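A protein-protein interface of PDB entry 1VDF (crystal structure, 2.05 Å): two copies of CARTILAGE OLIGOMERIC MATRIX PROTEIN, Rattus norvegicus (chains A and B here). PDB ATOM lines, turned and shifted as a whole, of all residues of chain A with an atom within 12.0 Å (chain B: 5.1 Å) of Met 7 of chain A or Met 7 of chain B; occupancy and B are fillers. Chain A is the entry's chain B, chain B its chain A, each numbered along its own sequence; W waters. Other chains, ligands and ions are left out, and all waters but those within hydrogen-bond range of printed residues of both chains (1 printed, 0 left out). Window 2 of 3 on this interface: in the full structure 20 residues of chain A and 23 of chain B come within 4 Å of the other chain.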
ATOM      1  N   MET A   1      -8.553  -1.831 -14.246  1.00  0.00           N
ATOM      2  CA  MET A   1      -9.127  -0.709 -13.515  1.00  0.00           C
ATOM      3  C   MET A   1      -9.444  -1.082 -12.057  1.00  0.00           C
ATOM      4  O   MET A   1      -9.598  -0.205 -11.200  1.00  0.00           O
ATOM      5  CB  MET A   1     -10.382  -0.173 -14.227  1.00  0.00           C
ATOM      6  CG  MET A   1     -11.691  -0.547 -13.534  1.00  0.00           C
ATOM      7  SD  MET A   1     -13.055   0.628 -13.810  1.00  0.00           S
ATOM      8  CE  MET A   1     -12.165   2.201 -13.698  1.00  0.00           C
ATOM      9  N   ASP A   2      -9.527  -2.397 -11.800  1.00  0.00           N
ATOM     10  CA  ASP A   2      -9.835  -2.975 -10.482  1.00  0.00           C
ATOM     11  C   ASP A   2      -9.218  -4.386 -10.449  1.00  0.00           C
ATOM     12  O   ASP A   2      -8.523  -4.791 -11.384  1.00  0.00           O
ATOM     13  CB  ASP A   2     -11.367  -3.173 -10.367  1.00  0.00           C
ATOM     14  CG  ASP A   2     -12.055  -2.158  -9.477  1.00  0.00           C
ATOM     15  OD1 ASP A   2     -11.413  -1.498  -8.654  1.00  0.00           O
ATOM     16  OD2 ASP A   2     -13.329  -2.073  -9.615  1.00  0.00           O
ATOM     17  N   LEU A   3      -9.539  -5.151  -9.395  1.00  0.00           N
ATOM     18  CA  LEU A   3      -9.097  -6.548  -9.238  1.00  0.00           C
ATOM     19  C   LEU A   3     -10.299  -7.498  -9.312  1.00  0.00           C
ATOM     20  O   LEU A   3     -10.206  -8.649  -8.923  1.00  0.00           O
ATOM     21  CB  LEU A   3      -8.435  -6.780  -7.866  1.00  0.00           C
ATOM     22  CG  LEU A   3      -7.142  -6.011  -7.635  1.00  0.00           C
ATOM     23  CD1 LEU A   3      -6.585  -6.374  -6.268  1.00  0.00           C
ATOM     24  CD2 LEU A   3      -6.150  -6.362  -8.724  1.00  0.00           C
ATOM     25  N   ALA A   4     -11.432  -6.995  -9.779  1.00  0.00           N
ATOM     26  CA  ALA A   4     -12.658  -7.781  -9.864  1.00  0.00           C
ATOM     27  C   ALA A   4     -12.551  -9.069 -10.687  1.00  0.00           C
ATOM     28  O   ALA A   4     -12.913 -10.149 -10.237  1.00  0.00           O
ATOM     29  CB  ALA A   4     -13.839  -6.909 -10.336  1.00  0.00           C
ATOM     30  N   PRO A   5     -12.059  -8.963 -11.900  1.00  0.00           N
ATOM     31  CA  PRO A   5     -11.968 -10.150 -12.702  1.00  0.00           C
ATOM     32  C   PRO A   5     -11.236 -11.235 -11.912  1.00  0.00           C
ATOM     33  O   PRO A   5     -11.650 -12.378 -11.929  1.00  0.00           O
ATOM     34  CB  PRO A   5     -11.183  -9.705 -13.935  1.00  0.00           C
ATOM     35  CG  PRO A   5     -11.351  -8.213 -14.022  1.00  0.00           C
ATOM     36  CD  PRO A   5     -11.594  -7.744 -12.612  1.00  0.00           C
ATOM     37  N   GLN A   6     -10.153 -10.865 -11.209  1.00  0.00           N
ATOM     38  CA  GLN A   6      -9.379 -11.826 -10.414  1.00  0.00           C
ATOM     39  C   GLN A   6     -10.178 -12.299  -9.226  1.00  0.00           C
ATOM     40  O   GLN A   6     -10.100 -13.466  -8.841  1.00  0.00           O
ATOM     41  CB  GLN A   6      -8.038 -11.238  -9.958  1.00  0.00           C
ATOM     42  CG  GLN A   6      -7.082 -11.010 -11.150  1.00  0.00           C
ATOM     43  CD  GLN A   6      -6.167  -9.807 -10.999  1.00  0.00           C
ATOM     44  OE1 GLN A   6      -4.986  -9.957 -10.668  1.00  0.00           O
ATOM     45  NE2 GLN A   6      -6.681  -8.621 -11.337  1.00  0.00           N
ATOM     46  N   MET A   7     -10.967 -11.382  -8.648  1.00  0.00           N
ATOM     47  CA  MET A   7     -11.808 -11.733  -7.509  1.00  0.00           C
ATOM     48  C   MET A   7     -12.909 -12.711  -7.894  1.00  0.00           C
ATOM     49  O   MET A   7     -13.129 -13.689  -7.193  1.00  0.00           O
ATOM     50  CB  MET A   7     -12.356 -10.512  -6.795  1.00  0.00           C
ATOM     51  CG  MET A   7     -11.298  -9.840  -5.935  1.00  0.00           C
ATOM     52  SD  MET A   7     -11.935  -8.523  -4.867  1.00  0.00           S
ATOM     53  CE  MET A   7     -12.561  -9.493  -3.468  1.00  0.00           C
ATOM     54  N   LEU A   8     -13.548 -12.447  -9.030  1.00  0.00           N
ATOM     55  CA  LEU A   8     -14.591 -13.293  -9.608  1.00  0.00           C
ATOM     56  C   LEU A   8     -14.023 -14.702  -9.823  1.00  0.00           C
ATOM     57  O   LEU A   8     -14.644 -15.684  -9.459  1.00  0.00           O
ATOM     58  CB  LEU A   8     -14.978 -12.705 -10.977  1.00  0.00           C
ATOM     59  CG  LEU A   8     -16.409 -12.818 -11.423  1.00  0.00           C
ATOM     60  CD1 LEU A   8     -16.412 -13.091 -12.915  1.00  0.00           C
ATOM     61  CD2 LEU A   8     -17.094 -13.942 -10.668  1.00  0.00           C
ATOM     62  N   ARG A   9     -12.815 -14.786 -10.401  1.00  0.00           N
ATOM     63  CA  ARG A   9     -12.150 -16.059 -10.638  1.00  0.00           C
ATOM     64  C   ARG A   9     -11.991 -16.888  -9.343  1.00  0.00           C
ATOM     65  O   ARG A   9     -12.329 -18.078  -9.294  1.00  0.00           O
ATOM     66  CB  ARG A   9     -10.824 -15.860 -11.408  1.00  0.00           C
ATOM     67  CG  ARG A   9      -9.827 -17.032 -11.425  1.00  0.00           C
ATOM     68  CD  ARG A   9     -10.438 -18.344 -11.940  1.00  0.00           C
ATOM     69  NE  ARG A   9      -9.499 -19.228 -12.650  1.00  0.00           N
ATOM     70  CZ  ARG A   9      -8.873 -20.270 -12.096  1.00  0.00           C
ATOM     71  NH1 ARG A   9      -9.042 -20.562 -10.803  1.00  0.00           N
ATOM     72  NH2 ARG A   9      -8.060 -21.018 -12.844  1.00  0.00           N
ATOM     73  N   GLU A  10     -11.516 -16.247  -8.288  1.00  0.00           N
ATOM     74  CA  GLU A  10     -11.359 -16.937  -7.017  1.00  0.00           C
ATOM     75  C   GLU A  10     -12.705 -17.388  -6.505  1.00  0.00           C
ATOM     76  O   GLU A  10     -12.840 -18.511  -6.034  1.00  0.00           O
ATOM     77  CB  GLU A  10     -10.710 -16.037  -5.963  1.00  0.00           C
ATOM     78  CG  GLU A  10      -9.235 -15.746  -6.201  1.00  0.00           C
ATOM     79  CD  GLU A  10      -8.400 -16.982  -6.403  1.00  0.00           C
ATOM     80  OE1 GLU A  10      -8.466 -17.924  -5.632  1.00  0.00           O
ATOM     81  OE2 GLU A  10      -7.600 -16.959  -7.386  1.00  0.00           O
ATOM     82  N   LEU A  11     -13.701 -16.514  -6.576  1.00  0.00           N
ATOM     83  CA  LEU A  11     -15.054 -16.870  -6.104  1.00  0.00           C
ATOM     84  C   LEU A  11     -15.604 -18.062  -6.887  1.00  0.00           C
ATOM     85  O   LEU A  11     -16.179 -18.999  -6.313  1.00  0.00           O
ATOM     86  CB  LEU A  11     -16.033 -15.667  -6.132  1.00  0.00           C
ATOM     87  CG  LEU A  11     -15.551 -14.490  -5.271  1.00  0.00           C
ATOM     88  CD1 LEU A  11     -16.442 -13.246  -5.440  1.00  0.00           C
ATOM     89  CD2 LEU A  11     -15.459 -14.939  -3.825  1.00  0.00           C
ATOM     90  N   GLN A  12     -15.406 -18.036  -8.198  1.00  0.00           N
ATOM     91  CA  GLN A  12     -15.868 -19.140  -9.025  1.00  0.00           C
ATOM     92  C   GLN A  12     -15.185 -20.427  -8.607  1.00  0.00           C
ATOM     93  O   GLN A  12     -15.827 -21.475  -8.544  1.00  0.00           O
ATOM     94  CB  GLN A  12     -15.641 -18.881 -10.517  1.00  0.00           C
ATOM     95  CG  GLN A  12     -16.551 -17.760 -11.046  1.00  0.00           C
ATOM     96  CD  GLN A  12     -16.141 -17.284 -12.437  1.00  0.00           C
ATOM     97  OE1 GLN A  12     -16.966 -16.794 -13.208  1.00  0.00           O
ATOM     98  NE2 GLN A  12     -14.864 -17.461 -12.764  1.00  0.00           N
ATOM     99  N   GLU A  13     -13.887 -20.354  -8.328  1.00  0.00           N
ATOM    100  CA  GLU A  13     -13.170 -21.558  -7.908  1.00  0.00           C
ATOM    101  C   GLU A  13     -13.589 -22.057  -6.518  1.00  0.00           C
ATOM    102  O   GLU A  13     -13.512 -23.244  -6.228  1.00  0.00           O
ATOM    103  CB  GLU A  13     -11.657 -21.391  -7.971  1.00  0.00           C
ATOM    104  CG  GLU A  13     -10.900 -22.693  -7.624  1.00  0.00           C
ATOM    105  CD  GLU A  13      -9.450 -22.446  -7.291  1.00  0.00           C
ATOM    106  OE1 GLU A  13      -8.824 -21.574  -8.006  1.00  0.00           O
ATOM    107  OE2 GLU A  13      -8.928 -23.054  -6.355  1.00  0.00           O
ATOM    108  N   THR A  14     -14.013 -21.149  -5.654  1.00  0.00           N
ATOM    109  CA  THR A  14     -14.461 -21.550  -4.332  1.00  0.00           C
ATOM    110  C   THR A  14     -15.723 -22.407  -4.495  1.00  0.00           C
ATOM    111  O   THR A  14     -15.879 -23.453  -3.873  1.00  0.00           O
ATOM    112  CB  THR A  14     -14.772 -20.304  -3.472  1.00  0.00           C
ATOM    113  OG1 THR A  14     -13.546 -19.754  -3.045  1.00  0.00           O
ATOM    114  CG2 THR A  14     -15.577 -20.662  -2.212  1.00  0.00           C
ATOM    115  N   ASN A  15     -16.611 -21.936  -5.355  1.00  0.00           N
ATOM    116  CA  ASN A  15     -17.866 -22.602  -5.644  1.00  0.00           C
ATOM    117  C   ASN A  15     -17.626 -23.961  -6.260  1.00  0.00           C
ATOM    118  O   ASN A  15     -18.118 -24.957  -5.776  1.00  0.00           O
ATOM    119  CB  ASN A  15     -18.755 -21.717  -6.528  1.00  0.00           C
ATOM    120  CG  ASN A  15     -19.344 -20.568  -5.753  1.00  0.00           C
ATOM    121  OD1 ASN A  15     -19.586 -20.678  -4.535  1.00  0.00           O
ATOM    122  ND2 ASN A  15     -19.550 -19.445  -6.430  1.00  0.00           N
ATOM    123  N   ALA A  16     -16.802 -24.021  -7.295  1.00  0.00           N
ATOM    124  CA  ALA A  16     -16.501 -25.311  -7.888  1.00  0.00           C
ATOM    125  C   ALA A  16     -16.030 -26.279  -6.804  1.00  0.00           C
ATOM    126  O   ALA A  16     -16.365 -27.459  -6.805  1.00  0.00           O
ATOM    127  CB  ALA A  16     -15.411 -25.157  -8.930  1.00  0.00           C
ATOM    128  N   LEU B   3      -7.567  -1.565   0.244  1.00  0.00           N
ATOM    129  CA  LEU B   3      -7.697  -2.941   0.679  1.00  0.00           C
ATOM    130  C   LEU B   3      -7.956  -4.024  -0.373  1.00  0.00           C
ATOM    131  O   LEU B   3      -7.941  -5.209  -0.021  1.00  0.00           O
ATOM    132  CB  LEU B   3      -8.810  -3.001   1.746  1.00  0.00           C
ATOM    133  CG  LEU B   3      -8.385  -2.712   3.174  1.00  0.00           C
ATOM    134  CD1 LEU B   3      -6.968  -2.110   3.249  1.00  0.00           C
ATOM    135  CD2 LEU B   3      -9.416  -1.854   3.882  1.00  0.00           C
ATOM    136  N   ALA B   4      -8.232  -3.656  -1.629  1.00  0.00           N
ATOM    137  CA  ALA B   4      -8.533  -4.656  -2.673  1.00  0.00           C
ATOM    138  C   ALA B   4      -7.562  -5.827  -2.733  1.00  0.00           C
ATOM    139  O   ALA B   4      -7.951  -6.984  -2.745  1.00  0.00           O
ATOM    140  CB  ALA B   4      -8.639  -4.011  -4.061  1.00  0.00           C
ATOM    141  N   PRO B   5      -6.278  -5.508  -2.813  1.00  0.00           N
ATOM    142  CA  PRO B   5      -5.249  -6.544  -2.915  1.00  0.00           C
ATOM    143  C   PRO B   5      -5.198  -7.530  -1.753  1.00  0.00           C
ATOM    144  O   PRO B   5      -5.019  -8.718  -1.993  1.00  0.00           O
ATOM    145  CB  PRO B   5      -3.935  -5.776  -3.093  1.00  0.00           C
ATOM    146  CG  PRO B   5      -4.324  -4.351  -3.441  1.00  0.00           C
ATOM    147  CD  PRO B   5      -5.729  -4.139  -2.923  1.00  0.00           C
ATOM    148  N   GLN B   6      -5.380  -7.032  -0.509  1.00  0.00           N
ATOM    149  CA  GLN B   6      -5.447  -7.872   0.695  1.00  0.00           C
ATOM    150  C   GLN B   6      -6.655  -8.819   0.638  1.00  0.00           C
ATOM    151  O   GLN B   6      -6.576  -9.962   1.065  1.00  0.00           O
ATOM    152  CB  GLN B   6      -5.560  -7.037   1.973  1.00  0.00           C
ATOM    153  CG  GLN B   6      -4.376  -6.097   2.221  1.00  0.00           C
ATOM    154  CD  GLN B   6      -4.255  -5.695   3.678  1.00  0.00           C
ATOM    155  OE1 GLN B   6      -4.568  -6.481   4.577  1.00  0.00           O
ATOM    156  NE2 GLN B   6      -3.810  -4.465   3.922  1.00  0.00           N
ATOM    157  N   MET B   7      -7.785  -8.332   0.113  1.00  0.00           N
ATOM    158  CA  MET B   7      -8.991  -9.163  -0.008  1.00  0.00           C
ATOM    159  C   MET B   7      -8.728 -10.295  -0.961  1.00  0.00           C
ATOM    160  O   MET B   7      -9.125 -11.429  -0.709  1.00  0.00           O
ATOM    161  CB  MET B   7     -10.210  -8.369  -0.536  1.00  0.00           C
ATOM    162  CG  MET B   7     -10.599  -7.205   0.384  1.00  0.00           C
ATOM    163  SD  MET B   7     -12.036  -6.212  -0.180  1.00  0.00           S
ATOM    164  CE  MET B   7     -13.315  -7.501  -0.252  1.00  0.00           C
ATOM    165  N   LEU B   8      -8.066  -9.970  -2.074  1.00  0.00           N
ATOM    166  CA  LEU B   8      -7.761 -10.955  -3.088  1.00  0.00           C
ATOM    167  C   LEU B   8      -6.874 -12.019  -2.485  1.00  0.00           C
ATOM    168  O   LEU B   8      -7.060 -13.201  -2.751  1.00  0.00           O
ATOM    169  CB  LEU B   8      -7.117 -10.315  -4.323  1.00  0.00           C
ATOM    170  CG  LEU B   8      -6.558 -11.289  -5.364  1.00  0.00           C
ATOM    171  CD1 LEU B   8      -7.669 -12.175  -5.884  1.00  0.00           C
ATOM    172  CD2 LEU B   8      -5.930 -10.500  -6.532  1.00  0.00           C
ATOM    173  N   ARG B   9      -5.931 -11.602  -1.647  1.00  0.00           N
ATOM    174  CA  ARG B   9      -5.040 -12.552  -0.996  1.00  0.00           C
ATOM    175  C   ARG B   9      -5.823 -13.541  -0.074  1.00  0.00           C
ATOM    176  O   ARG B   9      -5.521 -14.737  -0.017  1.00  0.00           O
ATOM    177  CB  ARG B   9      -3.983 -11.802  -0.180  1.00  0.00           C
ATOM    178  CG  ARG B   9      -2.707 -11.417  -0.941  1.00  0.00           C
ATOM    179  CD  ARG B   9      -1.919 -12.635  -1.467  1.00  0.00           C
ATOM    180  NE  ARG B   9      -1.243 -13.388  -0.405  1.00  0.00           N
ATOM    181  CZ  ARG B   9      -1.395 -14.689  -0.193  1.00  0.00           C
ATOM    182  NH1 ARG B   9      -2.187 -15.415  -0.974  1.00  0.00           N
ATOM    183  NH2 ARG B   9      -0.750 -15.267   0.807  1.00  0.00           N
ATOM    184  N   GLU B  10      -6.824 -13.041   0.652  1.00  0.00           N
ATOM    185  CA  GLU B  10      -7.628 -13.879   1.545  1.00  0.00           C
ATOM    186  C   GLU B  10      -8.435 -14.890   0.731  1.00  0.00           C
ATOM    187  O   GLU B  10      -8.602 -16.053   1.112  1.00  0.00           O
ATOM    188  CB  GLU B  10      -8.623 -13.023   2.350  1.00  0.00           C
ATOM    189  CG  GLU B  10      -7.978 -12.097   3.355  1.00  0.00           C
ATOM    190  CD  GLU B  10      -7.168 -12.854   4.358  1.00  0.00           C
ATOM    191  OE1 GLU B  10      -7.600 -13.895   4.872  1.00  0.00           O
ATOM    192  OE2 GLU B  10      -6.023 -12.375   4.607  1.00  0.00           O
ATOM    193  N   LEU B  11      -8.951 -14.442  -0.396  1.00  0.00           N
ATOM    194  CA  LEU B  11      -9.714 -15.342  -1.220  1.00  0.00           C
ATOM    195  C   LEU B  11      -8.853 -16.480  -1.730  1.00  0.00           C
ATOM    196  O   LEU B  11      -9.326 -17.600  -1.856  1.00  0.00           O
ATOM    197  CB  LEU B  11     -10.375 -14.618  -2.389  1.00  0.00           C
ATOM    198  CG  LEU B  11     -11.382 -13.533  -1.997  1.00  0.00           C
ATOM    199  CD1 LEU B  11     -11.910 -12.802  -3.234  1.00  0.00           C
ATOM    200  CD2 LEU B  11     -12.528 -14.109  -1.176  1.00  0.00           C
HETATM  201  O   HOH W   1     -12.185 -17.181  -2.659  1.00  0.00           O
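OG1 of Thr 14 of chain A lies within hydrogen-bond range of O of Glu 10 of chain A, at 3.3 Å.
Leu 3 of chain A touches Ala 4 of chain B (CD1 to C, 3.7 Å). Pro 5 of chain B touches Leu 3 of chain A. Met 7 of chain A touches Met 7 of chain B. Met 7 of chain A touches Leu 11 of chain B (CE to CD1, 3.4 Å). Leu 8 of chain B touches Glu 10 of chain A. Glu 10 of chain A touches Leu 11 of chain B.
Met 7 of chain A touches just these residues of chain B: Met 7 and Leu 11. No residue of chain A comes within 4 Å of Leu 3 of chain B. Ala 4 of chain B touches just one residue of chain A: Leu 3 (3.7 Å). No residue of chain A comes within 4 Å of Gln 6 of chain B. No residue of chain A comes within 4 Å of Glu 10 of chain B. Of chain A, only Met 7 (3.4 Å) and Glu 10 (3.9 Å) come within 4 Å of Leu 11 of chain B. Printed residues of chain B within 4 Å of Glu 10 of chain A: Leu 8 and Leu 11. Printed residues of chain B within 4 Å of Leu 3 of chain A: Ala 4 and Pro 5. Glu 13 of chain A touches none of the printed residues of chain B. Leu 11 of chain A touches none of the printed residues of chain B.
Among the printed residues, no Asp or Glu carboxylate lies within 4 Å of a Lys or Arg side-chain nitrogen of the other chain.
Leu 3 of chain A touches Ala 4 of chain B, but with the chains exchanged Ala 4 of chain A does not touch Leu 3 of chain B (10.5 Å). Leu 3 of chain A touches Pro 5 of chain B, but with the chains exchanged Pro 5 of chain A does not touch Leu 3 of chain B (13.1 Å). Met 7 of chain A touches its own counterpart, Met 7 of chain B. Glu 10 of chain A touches Leu 8 of chain B, but with the chains exchanged Leu 8 of chain A does not touch Glu 10 of chain B (11.3 Å). Positions printed for both chains: 3, 4, 5, 6, 7, 8, 9, 10 and 11.
Water W1 bridges OG1 of Thr 14 of chain A (2.9 Å) and O of Leu 11 of chain B (3.0 Å).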
